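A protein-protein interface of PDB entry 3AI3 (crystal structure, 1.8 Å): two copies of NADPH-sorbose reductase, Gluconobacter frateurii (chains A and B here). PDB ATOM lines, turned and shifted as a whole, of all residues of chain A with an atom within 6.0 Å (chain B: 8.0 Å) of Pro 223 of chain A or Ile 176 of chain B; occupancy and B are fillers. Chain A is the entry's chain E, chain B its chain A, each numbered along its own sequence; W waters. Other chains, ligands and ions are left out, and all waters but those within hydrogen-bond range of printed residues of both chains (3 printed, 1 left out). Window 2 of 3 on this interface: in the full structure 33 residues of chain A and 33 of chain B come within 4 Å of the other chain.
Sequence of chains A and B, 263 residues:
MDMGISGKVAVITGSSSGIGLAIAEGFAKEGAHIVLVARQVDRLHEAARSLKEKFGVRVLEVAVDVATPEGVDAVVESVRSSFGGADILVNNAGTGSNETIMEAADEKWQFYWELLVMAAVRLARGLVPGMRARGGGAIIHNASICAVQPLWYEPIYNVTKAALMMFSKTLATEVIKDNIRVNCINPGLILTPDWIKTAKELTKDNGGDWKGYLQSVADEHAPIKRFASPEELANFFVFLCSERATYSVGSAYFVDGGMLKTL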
ATOM      1  N   ALA A 218     -18.027   1.770 -17.441  1.00  0.00           N
ATOM      2  CA  ALA A 218     -16.649   1.644 -16.911  1.00  0.00           C
ATOM      3  C   ALA A 218     -15.942   2.989 -16.880  1.00  0.00           C
ATOM      4  O   ALA A 218     -15.334   3.346 -15.880  1.00  0.00           O
ATOM      5  CB  ALA A 218     -15.845   0.623 -17.703  1.00  0.00           C
ATOM      6  N   HIS A 221     -17.176   5.018 -13.846  1.00  0.00           N
ATOM      7  CA  HIS A 221     -16.981   4.551 -12.464  1.00  0.00           C
ATOM      8  C   HIS A 221     -15.566   4.097 -12.098  1.00  0.00           C
ATOM      9  O   HIS A 221     -15.167   4.192 -10.935  1.00  0.00           O
ATOM     10  CB  HIS A 221     -17.940   3.385 -12.173  1.00  0.00           C
ATOM     11  CG  HIS A 221     -19.384   3.787 -12.093  1.00  0.00           C
ATOM     12  ND1 HIS A 221     -19.869   4.629 -11.118  1.00  0.00           N
ATOM     13  CD2 HIS A 221     -20.451   3.434 -12.850  1.00  0.00           C
ATOM     14  CE1 HIS A 221     -21.168   4.799 -11.290  1.00  0.00           C
ATOM     15  NE2 HIS A 221     -21.549   4.076 -12.327  1.00  0.00           N
ATOM     16  N   ALA A 222     -14.830   3.544 -13.058  1.00  0.00           N
ATOM     17  CA  ALA A 222     -13.571   2.859 -12.712  1.00  0.00           C
ATOM     18  C   ALA A 222     -12.375   3.503 -13.400  1.00  0.00           C
ATOM     19  O   ALA A 222     -12.350   3.597 -14.634  1.00  0.00           O
ATOM     20  CB  ALA A 222     -13.659   1.389 -13.043  1.00  0.00           C
ATOM     21  N   PRO A 223     -11.373   3.951 -12.605  1.00  0.00           N
ATOM     22  CA  PRO A 223     -10.126   4.483 -13.138  1.00  0.00           C
ATOM     23  C   PRO A 223      -9.424   3.528 -14.116  1.00  0.00           C
ATOM     24  O   PRO A 223      -8.741   3.982 -15.030  1.00  0.00           O
ATOM     25  CB  PRO A 223      -9.278   4.671 -11.882  1.00  0.00           C
ATOM     26  CG  PRO A 223     -10.300   4.948 -10.805  1.00  0.00           C
ATOM     27  CD  PRO A 223     -11.450   4.081 -11.136  1.00  0.00           C
ATOM     28  N   ILE A 224      -9.589   2.218 -13.929  1.00  0.00           N
ATOM     29  CA  ILE A 224      -8.991   1.228 -14.830  1.00  0.00           C
ATOM     30  C   ILE A 224      -9.744   1.150 -16.190  1.00  0.00           C
ATOM     31  O   ILE A 224      -9.250   0.560 -17.159  1.00  0.00           O
ATOM     32  CB  ILE A 224      -8.924  -0.169 -14.139  1.00  0.00           C
ATOM     33  CG1 ILE A 224      -7.895  -1.085 -14.818  1.00  0.00           C
ATOM     34  CG2 ILE A 224     -10.351  -0.815 -14.060  1.00  0.00           C
ATOM     35  CD1 ILE A 224      -7.563  -2.366 -13.944  1.00  0.00           C
ATOM     36  N   LYS A 225     -10.931   1.741 -16.235  1.00  0.00           N
ATOM     37  CA  LYS A 225     -11.701   1.912 -17.480  1.00  0.00           C
ATOM     38  C   LYS A 225     -12.062   0.601 -18.176  1.00  0.00           C
ATOM     39  O   LYS A 225     -12.167   0.530 -19.424  1.00  0.00           O
ATOM     40  CB  LYS A 225     -10.956   2.849 -18.430  1.00  0.00           C
ATOM     41  CG  LYS A 225     -10.737   4.231 -17.823  1.00  0.00           C
ATOM     42  CD  LYS A 225     -10.118   5.192 -18.847  1.00  0.00           C
ATOM     43  CE  LYS A 225     -10.483   6.650 -18.528  1.00  0.00           C
ATOM     44  NZ  LYS A 225     -10.150   7.061 -17.135  1.00  0.00           N
ATOM     45  N   ARG A 226     -12.257  -0.435 -17.366  1.00  0.00           N
ATOM     46  CA  ARG A 226     -12.849  -1.682 -17.838  1.00  0.00           C
ATOM     47  C   ARG A 226     -13.553  -2.383 -16.683  1.00  0.00           C
ATOM     48  O   ARG A 226     -13.296  -2.073 -15.506  1.00  0.00           O
ATOM     49  CB  ARG A 226     -11.779  -2.624 -18.425  1.00  0.00           C
ATOM     50  CG  ARG A 226     -10.708  -3.040 -17.411  1.00  0.00           C
ATOM     51  CD  ARG A 226      -9.816  -4.086 -18.030  1.00  0.00           C
ATOM     52  NE  ARG A 226      -8.735  -4.516 -17.138  1.00  0.00           N
ATOM     53  CZ  ARG A 226      -8.866  -5.521 -16.276  1.00  0.00           C
ATOM     54  NH1 ARG A 226     -10.032  -6.155 -16.169  1.00  0.00           N
ATOM     55  NH2 ARG A 226      -7.846  -5.891 -15.526  1.00  0.00           N
ATOM     56  N   ASP A 256     -11.947  -3.594  -7.093  1.00  0.00           N
ATOM     57  CA  ASP A 256     -12.875  -2.670  -7.752  1.00  0.00           C
ATOM     58  C   ASP A 256     -12.290  -1.767  -8.823  1.00  0.00           C
ATOM     59  O   ASP A 256     -12.970  -0.847  -9.286  1.00  0.00           O
ATOM     60  CB  ASP A 256     -13.582  -1.796  -6.691  1.00  0.00           C
ATOM     61  CG  ASP A 256     -12.619  -0.899  -5.935  1.00  0.00           C
ATOM     62  OD1 ASP A 256     -11.522  -0.585  -6.453  1.00  0.00           O
ATOM     63  OD2 ASP A 256     -12.949  -0.521  -4.807  1.00  0.00           O
ATOM     64  N   GLY A 257     -11.046  -2.017  -9.221  1.00  0.00           N
ATOM     65  CA  GLY A 257     -10.455  -1.272 -10.338  1.00  0.00           C
ATOM     66  C   GLY A 257     -10.342   0.224 -10.095  1.00  0.00           C
ATOM     67  O   GLY A 257     -10.270   1.007 -11.046  1.00  0.00           O
ATOM     68  N   GLY A 258     -10.322   0.609  -8.818  1.00  0.00           N
ATOM     69  CA  GLY A 258     -10.230   2.013  -8.438  1.00  0.00           C
ATOM     70  C   GLY A 258     -11.544   2.701  -8.185  1.00  0.00           C
ATOM     71  O   GLY A 258     -11.558   3.905  -7.871  1.00  0.00           O
ATOM     72  N   MET A 259     -12.648   1.962  -8.313  1.00  0.00           N
ATOM     73  CA  MET A 259     -13.993   2.585  -8.226  1.00  0.00           C
ATOM     74  C   MET A 259     -14.314   3.275  -6.888  1.00  0.00           C
ATOM     75  O   MET A 259     -15.095   4.256  -6.846  1.00  0.00           O
ATOM     76  CB  MET A 259     -15.076   1.542  -8.515  1.00  0.00           C
ATOM     77  CG  MET A 259     -16.547   2.125  -8.586  1.00  0.00           C
ATOM     78  SD  MET A 259     -17.573   0.748  -9.210  1.00  0.00           S
ATOM     79  CE  MET A 259     -19.218   1.408  -8.931  1.00  0.00           C
ATOM     80  N   LEU A 260     -13.770   2.742  -5.799  1.00  0.00           N
ATOM     81  CA  LEU A 260     -14.012   3.327  -4.460  1.00  0.00           C
ATOM     82  C   LEU A 260     -13.322   4.676  -4.372  1.00  0.00           C
ATOM     83  O   LEU A 260     -12.105   4.758  -4.559  1.00  0.00           O
ATOM     84  CB  LEU A 260     -13.495   2.408  -3.341  1.00  0.00           C
ATOM     85  CG  LEU A 260     -13.748   2.907  -1.909  1.00  0.00           C
ATOM     86  CD1 LEU A 260     -15.258   2.972  -1.601  1.00  0.00           C
ATOM     87  CD2 LEU A 260     -12.997   2.040  -0.898  1.00  0.00           C
ATOM     88  N   GLY B 136       4.220  -1.847 -17.452  1.00  0.00           N
ATOM     89  CA  GLY B 136       3.360  -1.655 -16.296  1.00  0.00           C
ATOM     90  C   GLY B 136       4.020  -2.219 -15.059  1.00  0.00           C
ATOM     91  O   GLY B 136       5.197  -2.515 -15.059  1.00  0.00           O
ATOM     92  N   GLY B 137       3.257  -2.356 -13.987  1.00  0.00           N
ATOM     93  CA  GLY B 137       3.865  -2.869 -12.769  1.00  0.00           C
ATOM     94  C   GLY B 137       2.921  -2.848 -11.602  1.00  0.00           C
ATOM     95  O   GLY B 137       1.714  -2.614 -11.758  1.00  0.00           O
ATOM     96  N   LYS B 169      -3.293   5.923  -2.391  1.00  0.00           N
ATOM     97  CA  LYS B 169      -4.541   6.134  -3.146  1.00  0.00           C
ATOM     98  C   LYS B 169      -4.364   7.136  -4.267  1.00  0.00           C
ATOM     99  O   LYS B 169      -4.806   6.900  -5.403  1.00  0.00           O
ATOM    100  CB  LYS B 169      -5.669   6.581  -2.202  1.00  0.00           C
ATOM    101  CG  LYS B 169      -7.024   6.782  -2.898  1.00  0.00           C
ATOM    102  CD  LYS B 169      -7.500   5.551  -3.555  1.00  0.00           C
ATOM    103  CE  LYS B 169      -9.046   5.555  -3.651  1.00  0.00           C
ATOM    104  NZ  LYS B 169      -9.485   4.238  -4.170  1.00  0.00           N
ATOM    105  N   THR B 170      -3.684   8.239  -3.967  1.00  0.00           N
ATOM    106  CA  THR B 170      -3.464   9.278  -4.992  1.00  0.00           C
ATOM    107  C   THR B 170      -2.542   8.804  -6.092  1.00  0.00           C
ATOM    108  O   THR B 170      -2.748   9.145  -7.269  1.00  0.00           O
ATOM    109  CB  THR B 170      -2.938  10.620  -4.412  1.00  0.00           C
ATOM    110  OG1 THR B 170      -1.640  10.452  -3.855  1.00  0.00           O
ATOM    111  CG2 THR B 170      -3.906  11.161  -3.326  1.00  0.00           C
ATOM    112  N   LEU B 171      -1.526   8.021  -5.722  1.00  0.00           N
ATOM    113  CA  LEU B 171      -0.627   7.487  -6.727  1.00  0.00           C
ATOM    114  C   LEU B 171      -1.368   6.491  -7.612  1.00  0.00           C
ATOM    115  O   LEU B 171      -1.181   6.493  -8.839  1.00  0.00           O
ATOM    116  CB  LEU B 171       0.613   6.832  -6.091  1.00  0.00           C
ATOM    117  CG  LEU B 171       1.636   6.291  -7.088  1.00  0.00           C
ATOM    118  CD1 LEU B 171       2.270   7.481  -7.876  1.00  0.00           C
ATOM    119  CD2 LEU B 171       2.716   5.431  -6.395  1.00  0.00           C
ATOM    120  N   ALA B 172      -2.231   5.665  -7.006  1.00  0.00           N
ATOM    121  CA  ALA B 172      -2.970   4.657  -7.765  1.00  0.00           C
ATOM    122  C   ALA B 172      -3.776   5.292  -8.896  1.00  0.00           C
ATOM    123  O   ALA B 172      -3.784   4.763 -10.005  1.00  0.00           O
ATOM    124  CB  ALA B 172      -3.899   3.853  -6.878  1.00  0.00           C
ATOM    125  N   THR B 173      -4.427   6.412  -8.617  1.00  0.00           N
ATOM    126  CA  THR B 173      -5.268   7.020  -9.641  1.00  0.00           C
ATOM    127  C   THR B 173      -4.418   7.666 -10.730  1.00  0.00           C
ATOM    128  O   THR B 173      -4.809   7.687 -11.905  1.00  0.00           O
ATOM    129  CB  THR B 173      -6.355   7.943  -9.037  1.00  0.00           C
ATOM    130  OG1 THR B 173      -5.733   9.004  -8.318  1.00  0.00           O
ATOM    131  CG2 THR B 173      -7.255   7.146  -8.073  1.00  0.00           C
ATOM    132  N   GLU B 174      -3.228   8.131 -10.356  1.00  0.00           N
ATOM    133  CA  GLU B 174      -2.331   8.784 -11.293  1.00  0.00           C
ATOM    134  C   GLU B 174      -1.675   7.820 -12.282  1.00  0.00           C
ATOM    135  O   GLU B 174      -1.454   8.196 -13.437  1.00  0.00           O
ATOM    136  CB  GLU B 174      -1.214   9.550 -10.542  1.00  0.00           C
ATOM    137  CG  GLU B 174      -0.362  10.401 -11.453  1.00  0.00           C
ATOM    138  CD  GLU B 174       0.549  11.366 -10.720  1.00  0.00           C
ATOM    139  OE1 GLU B 174       0.081  12.019  -9.751  1.00  0.00           O
ATOM    140  OE2 GLU B 174       1.711  11.498 -11.162  1.00  0.00           O
ATOM    141  N   VAL B 175      -1.306   6.620 -11.828  1.00  0.00           N
ATOM    142  CA  VAL B 175      -0.466   5.739 -12.685  1.00  0.00           C
ATOM    143  C   VAL B 175      -1.196   4.530 -13.262  1.00  0.00           C
ATOM    144  O   VAL B 175      -0.597   3.746 -14.024  1.00  0.00           O
ATOM    145  CB  VAL B 175       0.859   5.329 -12.002  1.00  0.00           C
ATOM    146  CG1 VAL B 175       1.606   6.565 -11.517  1.00  0.00           C
ATOM    147  CG2 VAL B 175       0.585   4.381 -10.808  1.00  0.00           C
ATOM    148  N   ILE B 176      -2.494   4.379 -12.941  1.00  0.00           N
ATOM    149  CA  ILE B 176      -3.225   3.245 -13.500  1.00  0.00           C
ATOM    150  C   ILE B 176      -3.243   3.348 -15.046  1.00  0.00           C
ATOM    151  O   ILE B 176      -3.251   2.322 -15.718  1.00  0.00           O
ATOM    152  CB  ILE B 176      -4.664   3.001 -12.865  1.00  0.00           C
ATOM    153  CG1 ILE B 176      -5.315   1.710 -13.390  1.00  0.00           C
ATOM    154  CG2 ILE B 176      -5.619   4.148 -13.135  1.00  0.00           C
ATOM    155  CD1 ILE B 176      -4.563   0.394 -13.058  1.00  0.00           C
ATOM    156  N   LYS B 177      -3.210   4.574 -15.576  1.00  0.00           N
ATOM    157  CA  LYS B 177      -3.140   4.794 -17.028  1.00  0.00           C
ATOM    158  C   LYS B 177      -1.887   4.128 -17.645  1.00  0.00           C
ATOM    159  O   LYS B 177      -1.886   3.797 -18.857  1.00  0.00           O
ATOM    160  CB  LYS B 177      -3.171   6.294 -17.362  1.00  0.00           C
ATOM    161  CG  LYS B 177      -1.912   7.032 -16.924  1.00  0.00           C
ATOM    162  CD  LYS B 177      -1.919   8.517 -17.306  1.00  0.00           C
ATOM    163  CE  LYS B 177      -0.568   9.175 -16.939  1.00  0.00           C
ATOM    164  NZ  LYS B 177       0.643   8.694 -17.733  1.00  0.00           N
ATOM    165  N   ASP B 178      -0.852   3.912 -16.820  1.00  0.00           N
ATOM    166  CA  ASP B 178       0.391   3.258 -17.243  1.00  0.00           C
ATOM    167  C   ASP B 178       0.403   1.744 -16.997  1.00  0.00           C
ATOM    168  O   ASP B 178       1.460   1.093 -17.116  1.00  0.00           O
ATOM    169  CB  ASP B 178       1.599   3.868 -16.506  1.00  0.00           C
ATOM    170  CG  ASP B 178       1.739   5.349 -16.717  1.00  0.00           C
ATOM    171  OD1 ASP B 178       1.478   5.832 -17.845  1.00  0.00           O
ATOM    172  OD2 ASP B 178       2.149   6.021 -15.742  1.00  0.00           O
ATOM    173  N   ASN B 179      -0.759   1.178 -16.667  1.00  0.00           N
ATOM    174  CA  ASN B 179      -0.864  -0.225 -16.289  1.00  0.00           C
ATOM    175  C   ASN B 179      -0.026  -0.501 -15.044  1.00  0.00           C
ATOM    176  O   ASN B 179       0.529  -1.567 -14.902  1.00  0.00           O
ATOM    177  CB  ASN B 179      -0.447  -1.183 -17.450  1.00  0.00           C
ATOM    178  CG  ASN B 179      -0.787  -2.646 -17.166  1.00  0.00           C
ATOM    179  OD1 ASN B 179      -1.828  -2.962 -16.580  1.00  0.00           O
ATOM    180  ND2 ASN B 179       0.098  -3.553 -17.575  1.00  0.00           N
ATOM    181  N   ILE B 180       0.072   0.484 -14.161  1.00  0.00           N
ATOM    182  CA  ILE B 180       0.765   0.280 -12.889  1.00  0.00           C
ATOM    183  C   ILE B 180      -0.327   0.277 -11.813  1.00  0.00           C
ATOM    184  O   ILE B 180      -1.100   1.247 -11.690  1.00  0.00           O
ATOM    185  CB  ILE B 180       1.780   1.381 -12.609  1.00  0.00           C
ATOM    186  CG1 ILE B 180       2.903   1.352 -13.665  1.00  0.00           C
ATOM    187  CG2 ILE B 180       2.381   1.209 -11.169  1.00  0.00           C
ATOM    188  CD1 ILE B 180       3.788   2.586 -13.659  1.00  0.00           C
ATOM    189  N   ARG B 181      -0.382  -0.803 -11.045  1.00  0.00           N
ATOM    190  CA  ARG B 181      -1.419  -0.978 -10.028  1.00  0.00           C
ATOM    191  C   ARG B 181      -0.831  -0.716  -8.660  1.00  0.00           C
ATOM    192  O   ARG B 181       0.116  -1.372  -8.284  1.00  0.00           O
ATOM    193  CB  ARG B 181      -1.964  -2.403 -10.044  1.00  0.00           C
ATOM    194  CG  ARG B 181      -2.712  -2.802 -11.317  1.00  0.00           C
ATOM    195  CD  ARG B 181      -3.239  -4.246 -11.177  1.00  0.00           C
ATOM    196  NE  ARG B 181      -2.213  -5.283 -10.907  1.00  0.00           N
ATOM    197  CZ  ARG B 181      -1.912  -5.801  -9.704  1.00  0.00           C
ATOM    198  NH1 ARG B 181      -2.513  -5.358  -8.581  1.00  0.00           N
ATOM    199  NH2 ARG B 181      -0.977  -6.764  -9.605  1.00  0.00           N
ATOM    200  N   VAL B 182      -1.386   0.261  -7.945  1.00  0.00           N
ATOM    201  CA  VAL B 182      -0.879   0.669  -6.658  1.00  0.00           C
ATOM    202  C   VAL B 182      -1.879   0.351  -5.567  1.00  0.00           C
ATOM    203  O   VAL B 182      -3.056   0.707  -5.673  1.00  0.00           O
ATOM    204  CB  VAL B 182      -0.643   2.184  -6.626  1.00  0.00           C
ATOM    205  CG1 VAL B 182      -0.043   2.597  -5.261  1.00  0.00           C
ATOM    206  CG2 VAL B 182       0.264   2.609  -7.795  1.00  0.00           C
ATOM    207  N   THR B 246      -5.227  -8.494 -10.730  1.00  0.00           N
ATOM    208  CA  THR B 246      -5.149  -7.454 -11.760  1.00  0.00           C
ATOM    209  C   THR B 246      -6.275  -6.425 -11.734  1.00  0.00           C
ATOM    210  O   THR B 246      -6.277  -5.511 -12.549  1.00  0.00           O
ATOM    211  CB  THR B 246      -5.086  -8.097 -13.172  1.00  0.00           C
ATOM    212  OG1 THR B 246      -6.102  -9.110 -13.281  1.00  0.00           O
ATOM    213  CG2 THR B 246      -3.717  -8.716 -13.383  1.00  0.00           C
ATOM    214  N   TYR B 247      -7.223  -6.572 -10.808  1.00  0.00           N
ATOM    215  CA  TYR B 247      -8.305  -5.582 -10.669  1.00  0.00           C
ATOM    216  C   TYR B 247      -8.216  -4.824  -9.344  1.00  0.00           C
ATOM    217  O   TYR B 247      -9.089  -4.028  -9.011  1.00  0.00           O
ATOM    218  CB  TYR B 247      -9.672  -6.255 -10.817  1.00  0.00           C
ATOM    219  CG  TYR B 247     -10.707  -5.340 -11.392  1.00  0.00           C
ATOM    220  CD1 TYR B 247     -10.592  -4.862 -12.710  1.00  0.00           C
ATOM    221  CD2 TYR B 247     -11.807  -4.944 -10.626  1.00  0.00           C
ATOM    222  CE1 TYR B 247     -11.575  -4.019 -13.231  1.00  0.00           C
ATOM    223  CE2 TYR B 247     -12.789  -4.100 -11.151  1.00  0.00           C
ATOM    224  CZ  TYR B 247     -12.657  -3.646 -12.437  1.00  0.00           C
ATOM    225  OH  TYR B 247     -13.627  -2.814 -12.943  1.00  0.00           O
ATOM    226  N   SER B 248      -7.149  -5.086  -8.595  1.00  0.00           N
ATOM    227  CA  SER B 248      -6.890  -4.368  -7.350  1.00  0.00           C
ATOM    228  C   SER B 248      -6.185  -3.060  -7.688  1.00  0.00           C
ATOM    229  O   SER B 248      -5.030  -3.064  -8.115  1.00  0.00           O
ATOM    230  CB  SER B 248      -6.057  -5.242  -6.415  1.00  0.00           C
ATOM    231  OG  SER B 248      -6.848  -6.364  -6.019  1.00  0.00           O
ATOM    232  N   VAL B 249      -6.905  -1.946  -7.536  1.00  0.00           N
ATOM    233  CA  VAL B 249      -6.383  -0.610  -7.831  1.00  0.00           C
ATOM    234  C   VAL B 249      -6.794   0.378  -6.742  1.00  0.00           C
ATOM    235  O   VAL B 249      -7.981   0.611  -6.524  1.00  0.00           O
ATOM    236  CB  VAL B 249      -6.885  -0.077  -9.211  1.00  0.00           C
ATOM    237  CG1 VAL B 249      -6.375   1.325  -9.479  1.00  0.00           C
ATOM    238  CG2 VAL B 249      -6.428  -1.004 -10.303  1.00  0.00           C
ATOM    239  N   GLY B 250      -5.814   0.993  -6.095  1.00  0.00           N
ATOM    240  CA  GLY B 250      -6.122   2.045  -5.100  1.00  0.00           C
ATOM    241  C   GLY B 250      -6.833   1.568  -3.849  1.00  0.00           C
ATOM    242  O   GLY B 250      -7.611   2.315  -3.250  1.00  0.00           O
HETATM  243  O   HOH W   1      -9.501  -2.288  -6.059  1.00  0.00           O
HETATM  244  O   HOH W   2      -4.865  -4.651 -14.686  1.00  0.00           O
HETATM  245  O   HOH W   3     -14.993  -1.325 -11.030  1.00  0.00           O
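O of Gly 250 of chain B lies within hydrogen-bond range of NZ of Lys 169 of chain B.
O of Gly 257 of chain A lies within hydrogen-bond range of N of Ile 224 of chain A (3.2 Å).
The side-chain carboxylate (OD1) of Asp 256 of chain A lies within hydrogen-bond range of the backbone NH (N) of Gly 258 of chain A, at 2.9 Å.
The side-chain carboxylate (OD1) of Asp 256 of chain A sits at hydrogen-bond distance from the backbone NH (N) of Met 259 of chain A (3.3 Å).
Pro 223 of chain A touches Ile 176 of chain B.
Ile 224 of chain A touches Ile 176 of chain B.
Ile 224 of chain A touches Thr 246 of chain B.
CG2 of Ile 224 of chain A touches CE1 of Tyr 247 of chain B (3.5 Å).
Asp 256 of chain A touches Val 249 of chain B (OD1 to O, 3.7 Å).
Val 249 of chain B touches Gly 257 of chain A (CB to C, 3.6 Å).
Water W1 lies within hydrogen-bond range of OD1 of Asp 256 of chain A (2.7 Å), N of Val 249 of chain B (3.0 Å) and O of Tyr 247 of chain B (3.5 Å).
Water W2 bridges the backbone carbonyl oxygen of Thr 246 of chain B (2.7 Å) and the guanidinium group of Arg 226 of chain A (3.3 Å).
Water W3 lies within hydrogen-bond range of O of Asp 256 of chain A (2.7 Å), OH of Tyr 247 of chain B (2.8 Å) and SD of Met 259 of chain A (3.8 Å).
No position is printed for both chains.
Of the 12 pairs that touch across the chains among the printed residues, none has its exchanged pair printed and touching as well.
Of chain B, only Ile 176 (3.7 Å) comes within 4 Å of Pro 223 of chain A.
No residue of chain B comes within 4 Å of Ala 222 of chain A.
Of the printed residues of chain B, Ile 224 of chain A touches Ile 176, Thr 246 and Tyr 247.
Of the printed residues of chain A, Thr 246 of chain B touches Ile 224 and Arg 226.
Printed residues of chain B within 4 Å of Gly 258 of chain A: Val 249 (3.3 Å).
Of the printed residues of chain B, Leu 260 of chain A touches Lys 169.
The nearest residue of chain B that does not touch Pro 223 of chain A is Thr 173 of chain B (4.6 Å).
The nearest residue of chain A that does not touch Ile 176 of chain B is Gly 257 of chain A (5.5 Å).
Of the 12 printed residues of chain A, 7 touch a printed residue of chain B.
Hydrophobic or aromatic side chains of chain B within 4 Å of the printed part of chain A: Ile 176, Tyr 247 and Val 249.
Among the printed residues, 12 pairs touch across the chains.
O of Leu 260 of chain A lies within hydrogen-bond range of NZ of Lys 169 of chain B, at 2.7 Å.
NH2 of Arg 226 of chain A lies within hydrogen-bond range of O of Thr 246 of chain B, at 3.4 Å.
OH of Tyr 247 of chain B sits at hydrogen-bond distance from O of Arg 226 of chain A, 2.7 Å away.
The backbone carbonyl oxygen of Tyr 247 of chain B lies within hydrogen-bond range of the backbone NH of Asp 256 of chain A.
O of Tyr 247 of chain B sits at hydrogen-bond distance from N of Gly 257 of chain A (2.8 Å).
The backbone carbonyl oxygen (O) of Val 249 of chain B sits close to the backbone NH (N) of Gly 258 of chain A, at 3.3 Å.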
